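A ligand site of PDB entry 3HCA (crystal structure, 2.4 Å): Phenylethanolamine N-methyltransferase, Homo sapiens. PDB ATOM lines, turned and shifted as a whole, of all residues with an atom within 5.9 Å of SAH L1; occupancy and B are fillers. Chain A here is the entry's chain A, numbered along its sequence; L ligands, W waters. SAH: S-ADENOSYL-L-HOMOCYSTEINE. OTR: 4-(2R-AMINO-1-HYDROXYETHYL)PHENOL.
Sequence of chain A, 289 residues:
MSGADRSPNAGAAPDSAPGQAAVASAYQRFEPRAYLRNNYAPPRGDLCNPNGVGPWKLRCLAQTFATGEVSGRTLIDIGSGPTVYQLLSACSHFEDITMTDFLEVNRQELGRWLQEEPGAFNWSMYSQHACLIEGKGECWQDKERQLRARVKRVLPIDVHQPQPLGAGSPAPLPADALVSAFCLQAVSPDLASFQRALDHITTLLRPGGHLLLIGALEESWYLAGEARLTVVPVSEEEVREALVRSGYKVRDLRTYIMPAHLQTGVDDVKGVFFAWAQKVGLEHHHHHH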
ATOM      1  N   TYR A  27      23.987  26.065 -12.496  1.00  0.00           N
ATOM      2  CA  TYR A  27      24.463  26.867 -13.626  1.00  0.00           C
ATOM      3  C   TYR A  27      25.762  27.621 -13.318  1.00  0.00           C
ATOM      4  O   TYR A  27      26.352  28.238 -14.215  1.00  0.00           O
ATOM      5  CB  TYR A  27      23.390  27.856 -14.095  1.00  0.00           C
ATOM      6  CG  TYR A  27      22.477  27.282 -15.149  1.00  0.00           C
ATOM      7  CD1 TYR A  27      21.198  26.830 -14.819  1.00  0.00           C
ATOM      8  CD2 TYR A  27      22.885  27.175 -16.474  1.00  0.00           C
ATOM      9  CE1 TYR A  27      20.370  26.297 -15.770  1.00  0.00           C
ATOM     10  CE2 TYR A  27      22.049  26.645 -17.430  1.00  0.00           C
ATOM     11  CZ  TYR A  27      20.795  26.205 -17.076  1.00  0.00           C
ATOM     12  OH  TYR A  27      19.951  25.665 -18.024  1.00  0.00           O
ATOM     13  N   PHE A  30      28.344  25.764 -15.148  1.00  0.00           N
ATOM     14  CA  PHE A  30      28.105  25.739 -16.598  1.00  0.00           C
ATOM     15  C   PHE A  30      29.340  26.193 -17.384  1.00  0.00           C
ATOM     16  O   PHE A  30      29.839  27.298 -17.192  1.00  0.00           O
ATOM     17  CB  PHE A  30      26.916  26.652 -16.914  1.00  0.00           C
ATOM     18  CG  PHE A  30      26.526  26.671 -18.366  1.00  0.00           C
ATOM     19  CD1 PHE A  30      25.419  25.964 -18.808  1.00  0.00           C
ATOM     20  CD2 PHE A  30      27.237  27.419 -19.288  1.00  0.00           C
ATOM     21  CE1 PHE A  30      25.039  25.997 -20.141  1.00  0.00           C
ATOM     22  CE2 PHE A  30      26.871  27.450 -20.625  1.00  0.00           C
ATOM     23  CZ  PHE A  30      25.776  26.738 -21.050  1.00  0.00           C
ATOM     24  N   TYR A  35      29.410  23.326 -23.503  1.00  0.00           N
ATOM     25  CA  TYR A  35      28.056  23.384 -24.045  1.00  0.00           C
ATOM     26  C   TYR A  35      28.073  23.477 -25.561  1.00  0.00           C
ATOM     27  O   TYR A  35      27.314  22.785 -26.247  1.00  0.00           O
ATOM     28  CB  TYR A  35      27.282  24.552 -23.441  1.00  0.00           C
ATOM     29  CG  TYR A  35      25.905  24.726 -24.053  1.00  0.00           C
ATOM     30  CD1 TYR A  35      24.851  23.902 -23.681  1.00  0.00           C
ATOM     31  CD2 TYR A  35      25.666  25.714 -25.002  1.00  0.00           C
ATOM     32  CE1 TYR A  35      23.592  24.055 -24.240  1.00  0.00           C
ATOM     33  CE2 TYR A  35      24.409  25.877 -25.560  1.00  0.00           C
ATOM     34  CZ  TYR A  35      23.380  25.045 -25.174  1.00  0.00           C
ATOM     35  OH  TYR A  35      22.130  25.196 -25.729  1.00  0.00           O
ATOM     36  N   TYR A  40      26.916  22.087 -30.686  1.00  0.00           N
ATOM     37  CA  TYR A  40      27.139  22.833 -31.919  1.00  0.00           C
ATOM     38  C   TYR A  40      28.427  22.453 -32.630  1.00  0.00           C
ATOM     39  O   TYR A  40      28.904  23.164 -33.509  1.00  0.00           O
ATOM     40  CB  TYR A  40      27.031  24.329 -31.658  1.00  0.00           C
ATOM     41  CG  TYR A  40      25.660  24.690 -31.151  1.00  0.00           C
ATOM     42  CD1 TYR A  40      25.399  24.761 -29.791  1.00  0.00           C
ATOM     43  CD2 TYR A  40      24.602  24.889 -32.033  1.00  0.00           C
ATOM     44  CE1 TYR A  40      24.140  25.061 -29.325  1.00  0.00           C
ATOM     45  CE2 TYR A  40      23.334  25.192 -31.572  1.00  0.00           C
ATOM     46  CZ  TYR A  40      23.112  25.275 -30.214  1.00  0.00           C
ATOM     47  OH  TYR A  40      21.858  25.575 -29.757  1.00  0.00           O
ATOM     48  N   LYS A  57      16.599  23.721 -37.475  1.00  0.00           N
ATOM     49  CA  LYS A  57      16.393  24.915 -36.653  1.00  0.00           C
ATOM     50  C   LYS A  57      16.552  26.183 -37.477  1.00  0.00           C
ATOM     51  O   LYS A  57      15.786  27.134 -37.323  1.00  0.00           O
ATOM     52  CB  LYS A  57      17.353  24.939 -35.472  1.00  0.00           C
ATOM     53  CG  LYS A  57      17.074  23.877 -34.428  1.00  0.00           C
ATOM     54  CD  LYS A  57      17.882  24.119 -33.158  1.00  0.00           C
ATOM     55  CE  LYS A  57      19.377  23.999 -33.405  1.00  0.00           C
ATOM     56  NZ  LYS A  57      20.139  24.013 -32.125  1.00  0.00           N
ATOM     57  N   ASP A  77      17.082  38.732 -27.568  1.00  0.00           N
ATOM     58  CA  ASP A  77      17.362  37.302 -27.485  1.00  0.00           C
ATOM     59  C   ASP A  77      17.434  36.877 -26.023  1.00  0.00           C
ATOM     60  O   ASP A  77      18.302  37.322 -25.278  1.00  0.00           O
ATOM     61  CB  ASP A  77      18.678  36.987 -28.192  1.00  0.00           C
ATOM     62  CG  ASP A  77      18.856  35.495 -28.449  1.00  0.00           C
ATOM     63  OD1 ASP A  77      17.840  34.789 -28.626  1.00  0.00           O
ATOM     64  OD2 ASP A  77      20.014  35.031 -28.469  1.00  0.00           O
ATOM     65  N   ILE A  78      16.500  36.021 -25.609  1.00  0.00           N
ATOM     66  CA  ILE A  78      16.407  35.569 -24.226  1.00  0.00           C
ATOM     67  C   ILE A  78      17.325  34.374 -23.989  1.00  0.00           C
ATOM     68  O   ILE A  78      17.255  33.393 -24.710  1.00  0.00           O
ATOM     69  CB  ILE A  78      14.974  35.148 -23.878  1.00  0.00           C
ATOM     70  CG1 ILE A  78      13.975  36.229 -24.307  1.00  0.00           C
ATOM     71  CG2 ILE A  78      14.848  34.846 -22.399  1.00  0.00           C
ATOM     72  CD1 ILE A  78      14.272  37.601 -23.735  1.00  0.00           C
ATOM     73  N   GLY A  79      18.167  34.472 -22.962  1.00  0.00           N
ATOM     74  CA  GLY A  79      19.092  33.398 -22.631  1.00  0.00           C
ATOM     75  C   GLY A  79      19.904  32.931 -23.828  1.00  0.00           C
ATOM     76  O   GLY A  79      19.870  31.757 -24.200  1.00  0.00           O
ATOM     77  N   SER A  80      20.639  33.861 -24.419  1.00  0.00           N
ATOM     78  CA  SER A  80      21.416  33.588 -25.624  1.00  0.00           C
ATOM     79  C   SER A  80      22.493  32.546 -25.404  1.00  0.00           C
ATOM     80  O   SER A  80      22.887  31.828 -26.328  1.00  0.00           O
ATOM     81  CB  SER A  80      22.071  34.875 -26.122  1.00  0.00           C
ATOM     82  OG  SER A  80      21.143  35.939 -26.193  1.00  0.00           O
ATOM     83  N   GLY A  81      22.980  32.450 -24.172  1.00  0.00           N
ATOM     84  CA  GLY A  81      24.115  31.595 -23.897  1.00  0.00           C
ATOM     85  C   GLY A  81      25.265  32.075 -24.752  1.00  0.00           C
ATOM     86  O   GLY A  81      25.389  33.263 -25.014  1.00  0.00           O
ATOM     87  N   PRO A  82      26.105  31.143 -25.205  1.00  0.00           N
ATOM     88  CA  PRO A  82      27.259  31.497 -26.046  1.00  0.00           C
ATOM     89  C   PRO A  82      27.003  31.264 -27.529  1.00  0.00           C
ATOM     90  O   PRO A  82      27.953  31.074 -28.276  1.00  0.00           O
ATOM     91  CB  PRO A  82      28.318  30.528 -25.540  1.00  0.00           C
ATOM     92  CG  PRO A  82      27.531  29.265 -25.262  1.00  0.00           C
ATOM     93  CD  PRO A  82      26.124  29.717 -24.854  1.00  0.00           C
ATOM     94  N   THR A  83      25.738  31.279 -27.954  1.00  0.00           N
ATOM     95  CA  THR A  83      25.407  30.968 -29.340  1.00  0.00           C
ATOM     96  C   THR A  83      24.727  32.137 -30.051  1.00  0.00           C
ATOM     97  O   THR A  83      24.072  32.956 -29.416  1.00  0.00           O
ATOM     98  CB  THR A  83      24.487  29.726 -29.431  1.00  0.00           C
ATOM     99  OG1 THR A  83      23.155  30.082 -29.040  1.00  0.00           O
ATOM    100  CG2 THR A  83      25.010  28.611 -28.533  1.00  0.00           C
ATOM    101  N   TYR A  85      23.614  31.525 -33.649  1.00  0.00           N
ATOM    102  CA  TYR A  85      22.943  30.954 -34.822  1.00  0.00           C
ATOM    103  C   TYR A  85      21.486  31.386 -34.851  1.00  0.00           C
ATOM    104  O   TYR A  85      20.891  31.529 -35.926  1.00  0.00           O
ATOM    105  CB  TYR A  85      23.016  29.431 -34.794  1.00  0.00           C
ATOM    106  CG  TYR A  85      22.082  28.823 -33.777  1.00  0.00           C
ATOM    107  CD1 TYR A  85      20.813  28.409 -34.137  1.00  0.00           C
ATOM    108  CD2 TYR A  85      22.462  28.707 -32.444  1.00  0.00           C
ATOM    109  CE1 TYR A  85      19.943  27.879 -33.198  1.00  0.00           C
ATOM    110  CE2 TYR A  85      21.606  28.175 -31.509  1.00  0.00           C
ATOM    111  CZ  TYR A  85      20.346  27.761 -31.887  1.00  0.00           C
ATOM    112  OH  TYR A  85      19.492  27.238 -30.951  1.00  0.00           O
ATOM    113  N   GLN A  86      20.902  31.580 -33.677  1.00  0.00           N
ATOM    114  CA  GLN A  86      19.474  31.845 -33.565  1.00  0.00           C
ATOM    115  C   GLN A  86      19.081  33.248 -33.995  1.00  0.00           C
ATOM    116  O   GLN A  86      17.914  33.608 -33.946  1.00  0.00           O
ATOM    117  CB  GLN A  86      18.970  31.569 -32.132  1.00  0.00           C
ATOM    118  CG  GLN A  86      19.497  32.535 -31.072  1.00  0.00           C
ATOM    119  CD  GLN A  86      20.823  32.105 -30.477  1.00  0.00           C
ATOM    120  OE1 GLN A  86      21.527  31.268 -31.039  1.00  0.00           O
ATOM    121  NE2 GLN A  86      21.179  32.676 -29.327  1.00  0.00           N
ATOM    122  N   ASP A 101      22.005  37.005 -21.275  1.00  0.00           N
ATOM    123  CA  ASP A 101      22.219  35.734 -20.578  1.00  0.00           C
ATOM    124  C   ASP A 101      22.462  35.928 -19.092  1.00  0.00           C
ATOM    125  O   ASP A 101      22.992  36.946 -18.656  1.00  0.00           O
ATOM    126  CB  ASP A 101      23.364  34.919 -21.186  1.00  0.00           C
ATOM    127  CG  ASP A 101      23.280  33.449 -20.799  1.00  0.00           C
ATOM    128  OD1 ASP A 101      22.335  32.769 -21.244  1.00  0.00           O
ATOM    129  OD2 ASP A 101      24.158  32.975 -20.049  1.00  0.00           O
ATOM    130  N   PHE A 102      22.073  34.921 -18.313  1.00  0.00           N
ATOM    131  CA  PHE A 102      22.199  34.950 -16.868  1.00  0.00           C
ATOM    132  C   PHE A 102      23.655  34.870 -16.418  1.00  0.00           C
ATOM    133  O   PHE A 102      24.025  35.409 -15.375  1.00  0.00           O
ATOM    134  CB  PHE A 102      21.391  33.789 -16.283  1.00  0.00           C
ATOM    135  CG  PHE A 102      21.467  33.680 -14.796  1.00  0.00           C
ATOM    136  CD1 PHE A 102      20.634  34.433 -13.974  1.00  0.00           C
ATOM    137  CD2 PHE A 102      22.359  32.798 -14.198  1.00  0.00           C
ATOM    138  CE1 PHE A 102      20.702  34.318 -12.606  1.00  0.00           C
ATOM    139  CE2 PHE A 102      22.426  32.674 -12.830  1.00  0.00           C
ATOM    140  CZ  PHE A 102      21.596  33.439 -12.029  1.00  0.00           C
ATOM    141  N   LEU A 103      24.489  34.207 -17.217  1.00  0.00           N
ATOM    142  CA  LEU A 103      25.886  33.974 -16.845  1.00  0.00           C
ATOM    143  C   LEU A 103      26.875  34.956 -17.468  1.00  0.00           C
ATOM    144  O   LEU A 103      26.820  35.233 -18.670  1.00  0.00           O
ATOM    145  CB  LEU A 103      26.308  32.544 -17.196  1.00  0.00           C
ATOM    146  CG  LEU A 103      25.655  31.417 -16.402  1.00  0.00           C
ATOM    147  CD1 LEU A 103      26.143  30.062 -16.900  1.00  0.00           C
ATOM    148  CD2 LEU A 103      25.937  31.583 -14.917  1.00  0.00           C
ATOM    149  N   ASN A 106      29.140  33.392 -20.244  1.00  0.00           N
ATOM    150  CA  ASN A 106      28.468  33.350 -21.531  1.00  0.00           C
ATOM    151  C   ASN A 106      28.452  34.712 -22.222  1.00  0.00           C
ATOM    152  O   ASN A 106      28.686  34.803 -23.426  1.00  0.00           O
ATOM    153  CB  ASN A 106      27.043  32.798 -21.395  1.00  0.00           C
ATOM    154  CG  ASN A 106      27.018  31.296 -21.284  1.00  0.00           C
ATOM    155  OD1 ASN A 106      26.074  30.717 -20.750  1.00  0.00           O
ATOM    156  ND2 ASN A 106      28.067  30.641 -21.761  1.00  0.00           N
ATOM    157  N   ILE A 157      20.344  38.820 -17.453  1.00  0.00           N
ATOM    158  CA  ILE A 157      18.905  38.604 -17.439  1.00  0.00           C
ATOM    159  C   ILE A 157      18.541  37.433 -16.533  1.00  0.00           C
ATOM    160  O   ILE A 157      19.312  36.470 -16.422  1.00  0.00           O
ATOM    161  CB  ILE A 157      18.359  38.334 -18.862  1.00  0.00           C
ATOM    162  CG1 ILE A 157      16.834  38.272 -18.849  1.00  0.00           C
ATOM    163  CG2 ILE A 157      18.953  37.057 -19.428  1.00  0.00           C
ATOM    164  CD1 ILE A 157      16.214  38.084 -20.221  1.00  0.00           C
ATOM    165  N   ASP A 158      17.384  37.506 -15.898  1.00  0.00           N
ATOM    166  CA  ASP A 158      16.861  36.411 -15.090  1.00  0.00           C
ATOM    167  C   ASP A 158      15.373  36.261 -15.364  1.00  0.00           C
ATOM    168  O   ASP A 158      14.567  37.060 -14.891  1.00  0.00           O
ATOM    169  CB  ASP A 158      17.113  36.666 -13.610  1.00  0.00           C
ATOM    170  CG  ASP A 158      16.663  35.516 -12.729  1.00  0.00           C
ATOM    171  OD1 ASP A 158      16.081  34.542 -13.261  1.00  0.00           O
ATOM    172  OD2 ASP A 158      16.884  35.582 -11.505  1.00  0.00           O
ATOM    173  N   VAL A 159      15.016  35.245 -16.138  1.00  0.00           N
ATOM    174  CA  VAL A 159      13.624  35.037 -16.531  1.00  0.00           C
ATOM    175  C   VAL A 159      12.746  34.704 -15.324  1.00  0.00           C
ATOM    176  O   VAL A 159      11.515  34.654 -15.435  1.00  0.00           O
ATOM    177  CB  VAL A 159      13.497  33.932 -17.579  1.00  0.00           C
ATOM    178  CG1 VAL A 159      14.223  34.337 -18.858  1.00  0.00           C
ATOM    179  CG2 VAL A 159      14.039  32.617 -17.035  1.00  0.00           C
ATOM    180  N   HIS A 160      13.371  34.474 -14.176  1.00  0.00           N
ATOM    181  CA  HIS A 160      12.635  34.141 -12.972  1.00  0.00           C
ATOM    182  C   HIS A 160      12.111  35.375 -12.254  1.00  0.00           C
ATOM    183  O   HIS A 160      11.291  35.279 -11.334  1.00  0.00           O
ATOM    184  CB  HIS A 160      13.481  33.291 -12.034  1.00  0.00           C
ATOM    185  CG  HIS A 160      13.845  31.950 -12.599  1.00  0.00           C
ATOM    186  ND1 HIS A 160      12.892  31.083 -13.106  1.00  0.00           N
ATOM    187  CD2 HIS A 160      15.035  31.328 -12.738  1.00  0.00           C
ATOM    188  CE1 HIS A 160      13.494  29.984 -13.530  1.00  0.00           C
ATOM    189  NE2 HIS A 160      14.791  30.111 -13.326  1.00  0.00           N
ATOM    190  N   SER A 180      13.833  33.116 -28.220  1.00  0.00           N
ATOM    191  CA  SER A 180      14.324  32.360 -27.077  1.00  0.00           C
ATOM    192  C   SER A 180      14.548  30.903 -27.445  1.00  0.00           C
ATOM    193  O   SER A 180      13.594  30.174 -27.725  1.00  0.00           O
ATOM    194  CB  SER A 180      13.346  32.465 -25.913  1.00  0.00           C
ATOM    195  OG  SER A 180      13.795  31.702 -24.804  1.00  0.00           O
ATOM    196  N   ALA A 181      15.801  30.477 -27.447  1.00  0.00           N
ATOM    197  CA  ALA A 181      16.146  29.107 -27.818  1.00  0.00           C
ATOM    198  C   ALA A 181      16.794  28.337 -26.669  1.00  0.00           C
ATOM    199  O   ALA A 181      17.847  28.719 -26.165  1.00  0.00           O
ATOM    200  CB  ALA A 181      17.060  29.103 -29.028  1.00  0.00           C
ATOM    201  N   PHE A 182      16.152  27.244 -26.267  1.00  0.00           N
ATOM    202  CA  PHE A 182      16.697  26.367 -25.243  1.00  0.00           C
ATOM    203  C   PHE A 182      16.987  27.109 -23.947  1.00  0.00           C
ATOM    204  O   PHE A 182      18.040  26.921 -23.329  1.00  0.00           O
ATOM    205  CB  PHE A 182      17.958  25.671 -25.765  1.00  0.00           C
ATOM    206  CG  PHE A 182      17.739  24.900 -27.033  1.00  0.00           C
ATOM    207  CD1 PHE A 182      18.215  25.382 -28.243  1.00  0.00           C
ATOM    208  CD2 PHE A 182      17.054  23.697 -27.019  1.00  0.00           C
ATOM    209  CE1 PHE A 182      18.022  24.677 -29.417  1.00  0.00           C
ATOM    210  CE2 PHE A 182      16.846  22.985 -28.191  1.00  0.00           C
ATOM    211  CZ  PHE A 182      17.332  23.474 -29.394  1.00  0.00           C
ATOM    212  N   CYS A 183      16.043  27.943 -23.527  1.00  0.00           N
ATOM    213  CA  CYS A 183      16.205  28.700 -22.289  1.00  0.00           C
ATOM    214  C   CYS A 183      15.166  28.375 -21.215  1.00  0.00           C
ATOM    215  O   CYS A 183      15.486  27.783 -20.188  1.00  0.00           O
ATOM    216  CB  CYS A 183      16.211  30.205 -22.581  1.00  0.00           C
ATOM    217  SG  CYS A 183      16.386  31.176 -21.086  1.00  0.00           S
ATOM    218  N   ALA A 186      14.915  24.998 -20.146  1.00  0.00           N
ATOM    219  CA  ALA A 186      16.246  24.641 -19.651  1.00  0.00           C
ATOM    220  C   ALA A 186      16.566  25.257 -18.304  1.00  0.00           C
ATOM    221  O   ALA A 186      17.578  24.924 -17.686  1.00  0.00           O
ATOM    222  CB  ALA A 186      17.313  25.016 -20.687  1.00  0.00           C
ATOM    223  N   VAL A 187      15.705  26.160 -17.827  1.00  0.00           N
ATOM    224  CA  VAL A 187      15.917  26.817 -16.540  1.00  0.00           C
ATOM    225  C   VAL A 187      14.748  26.596 -15.581  1.00  0.00           C
ATOM    226  O   VAL A 187      14.638  27.262 -14.560  1.00  0.00           O
ATOM    227  CB  VAL A 187      16.160  28.328 -16.703  1.00  0.00           C
ATOM    228  CG1 VAL A 187      17.314  28.585 -17.680  1.00  0.00           C
ATOM    229  CG2 VAL A 187      14.893  29.020 -17.186  1.00  0.00           C
ATOM    230  N   TYR A 222      20.657  17.795 -19.225  1.00  0.00           N
ATOM    231  CA  TYR A 222      21.705  17.964 -20.225  1.00  0.00           C
ATOM    232  C   TYR A 222      22.979  18.454 -19.556  1.00  0.00           C
ATOM    233  O   TYR A 222      22.928  19.137 -18.525  1.00  0.00           O
ATOM    234  CB  TYR A 222      21.256  18.915 -21.346  1.00  0.00           C
ATOM    235  CG  TYR A 222      21.341  20.380 -21.003  1.00  0.00           C
ATOM    236  CD1 TYR A 222      22.467  21.121 -21.313  1.00  0.00           C
ATOM    237  CD2 TYR A 222      20.279  21.031 -20.374  1.00  0.00           C
ATOM    238  CE1 TYR A 222      22.549  22.467 -21.006  1.00  0.00           C
ATOM    239  CE2 TYR A 222      20.356  22.377 -20.058  1.00  0.00           C
ATOM    240  CZ  TYR A 222      21.496  23.096 -20.383  1.00  0.00           C
ATOM    241  OH  TYR A 222      21.583  24.442 -20.085  1.00  0.00           O
HETATM  242  N   SAH L   1      20.200  29.926 -26.400  1.00  0.00           N
HETATM  243  CA  SAH L   1      21.359  29.071 -26.601  1.00  0.00           C
HETATM  244  CB  SAH L   1      21.972  28.616 -25.267  1.00  0.00           C
HETATM  245  CG  SAH L   1      20.925  28.097 -24.277  1.00  0.00           C
HETATM  246  SD  SAH L   1      21.740  27.408 -22.810  1.00  0.00           S
HETATM  247  C   SAH L   1      20.992  27.873 -27.473  1.00  0.00           C
HETATM  248  O   SAH L   1      21.768  26.982 -27.461  1.00  0.00           O
HETATM  249  OXT SAH L   1      20.051  28.114 -28.485  1.00  0.00           O
HETATM  250  C5' SAH L   1      20.672  28.040 -21.490  1.00  0.00           C
HETATM  251  C4' SAH L   1      21.073  29.402 -20.941  1.00  0.00           C
HETATM  252  O4' SAH L   1      20.187  29.765 -19.943  1.00  0.00           O
HETATM  253  C3' SAH L   1      22.443  29.346 -20.277  1.00  0.00           C
HETATM  254  O3' SAH L   1      23.323  30.204 -20.959  1.00  0.00           O
HETATM  255  C2' SAH L   1      22.203  29.781 -18.984  1.00  0.00           C
HETATM  256  O2' SAH L   1      23.249  30.590 -18.507  1.00  0.00           O
HETATM  257  C1' SAH L   1      20.970  30.500 -19.062  1.00  0.00           C
HETATM  258  N9  SAH L   1      20.290  30.704 -17.792  1.00  0.00           N
HETATM  259  C8  SAH L   1      20.494  30.012 -16.669  1.00  0.00           C
HETATM  260  N7  SAH L   1      19.629  30.530 -15.716  1.00  0.00           N
HETATM  261  C5  SAH L   1      18.897  31.538 -16.285  1.00  0.00           C
HETATM  262  C6  SAH L   1      17.915  32.373 -15.794  1.00  0.00           C
HETATM  263  N6  SAH L   1      17.491  32.250 -14.408  1.00  0.00           N
HETATM  264  N1  SAH L   1      17.357  33.299 -16.597  1.00  0.00           N
HETATM  265  C2  SAH L   1      17.776  33.391 -17.883  1.00  0.00           C
HETATM  266  N3  SAH L   1      18.742  32.569 -18.360  1.00  0.00           N
HETATM  267  C4  SAH L   1      19.294  31.654 -17.560  1.00  0.00           C
HETATM  268  C2  OTR L   2      20.390  21.936 -27.210  1.00  0.00           C
HETATM  269  C3  OTR L   2      20.681  21.870 -28.577  1.00  0.00           C
HETATM  270  C4  OTR L   2      20.340  20.721 -29.297  1.00  0.00           C
HETATM  271  O4  OTR L   2      20.632  20.623 -30.664  1.00  0.00           O
HETATM  272  C5  OTR L   2      19.706  19.650 -28.663  1.00  0.00           C
HETATM  273  C6  OTR L   2      19.414  19.729 -27.308  1.00  0.00           C
HETATM  274  C1  OTR L   2      19.753  20.868 -26.589  1.00  0.00           C
HETATM  275  C7  OTR L   2      19.405  20.932 -25.094  1.00  0.00           C
HETATM  276  O7  OTR L   2      20.112  19.972 -24.368  1.00  0.00           O
HETATM  277  C8  OTR L   2      19.696  22.319 -24.548  1.00  0.00           C
HETATM  278  N8  OTR L   2      19.017  22.439 -23.278  1.00  0.00           N
HETATM  279  O   HOH W   1      19.854  24.899 -22.879  1.00  0.00           O
HETATM  280  O   HOH W   2      18.267  32.435 -27.177  1.00  0.00           O
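The backbone carbonyl oxygen (O) of Phe 182 sits close to a sulfur (SD) of SAH L1 (3.8 Å).
Tyr 27 touches SAH L1.
Gly 81 touches SAH L1.
Thr 83 touches SAH L1.
Phe 102 touches SAH L1.
CG of Leu 103 touches O2' of SAH L1 (3.3 Å).
Ile 157 touches SAH L1 (O to N1, 3.7 Å).
His 160 touches SAH L1.
Cys 183 touches SAH L1 (SG to N3, 3.9 Å).
Val 187 touches SAH L1 (CG1 to N7, 3.6 Å).
Tyr 222 touches SAH L1.
Hydrophobic or aromatic side chains that line SAH L1: Tyr 27, Tyr 35, Tyr 40, Tyr 85, Phe 102, Leu 103, Val 159, His 160, Ala 181, Phe 182 and Val 187.
Within 4 Å of SAH L1: Tyr 27, Tyr 35, Tyr 40, Gly 79, Ser 80, Gly 81, Thr 83, Tyr 85, Asp 101, Phe 102, Leu 103, Asn 106, Ile 157, Asp 158, Val 159, His 160, Ala 181, Phe 182, Cys 183, Val 187 and Tyr 222.
The nearest printed residue that does not touch SAH L1 is Gln 86 (4.1 Å).
OH of Tyr 85 sits at hydrogen-bond distance from NZ of Lys 57 (3.5 Å).
The side-chain hydroxyl (OH) of Tyr 40 is in hydrogen-bond range of the side-chain amino group (NZ) of Lys 57, at 3.3 Å.
The backbone NH of Leu 103 is in hydrogen-bond range of the side-chain carboxylate of Asp 101 (3.1 Å).
The side-chain carboxylate (OD1) of Asp 101 is in hydrogen-bond range of the backbone NH (N) of Gly 81.
The side-chain carboxylate (OD1) of Asp 158 lies within hydrogen-bond range of the backbone NH (N) of His 160 (2.9 Å).
The backbone carbonyl oxygen of Ser 80 sits at hydrogen-bond distance from the side-chain hydroxyl of Thr 83.
OH of Tyr 222 is in hydrogen-bond range of OH of Tyr 27.
The backbone carbonyl oxygen (O) of Ala 186 is in hydrogen-bond range of the side-chain hydroxyl (OH) of Tyr 27, at 2.5 Å.
The side-chain hydroxyl of Tyr 35 is in hydrogen-bond range of an oxygen (O) of SAH L1 (2.5 Å).
The backbone carbonyl oxygen of Ala 181 sits at hydrogen-bond distance from a nitrogen (N) of SAH L1, at 2.7 Å.
An oxygen (OXT) of SAH L1 sits at hydrogen-bond distance from the side-chain hydroxyl (OH) of Tyr 85 (2.7 Å).
O of SAH L1 is in hydrogen-bond range of OH of Tyr 40 (2.7 Å).
The side-chain carboxylate (OD1) of Asp 101 sits at hydrogen-bond distance from an oxygen (O3') of SAH L1, 2.8 Å away.
The side-chain amide oxygen of Asn 106 sits at hydrogen-bond distance from an oxygen (O3') of SAH L1, 2.8 Å away.
N of SAH L1 lies within hydrogen-bond range of O of Gly 79 (2.9 Å).
The side-chain carboxylate (OD1) of Asp 158 is in hydrogen-bond range of a nitrogen (N6) of SAH L1 (2.9 Å).
N of Val 159 lies within hydrogen-bond range of N1 of SAH L1, 3.1 Å away.
The backbone carbonyl oxygen of Ser 80 sits close to a nitrogen (N) of SAH L1 (3.3 Å).
Water W1 lies within hydrogen-bond range of N8 of OTR L2 (2.6 Å), O of Phe 182 (2.8 Å), SD of SAH L1 (3.1 Å) and OH of Tyr 222 (3.3 Å).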
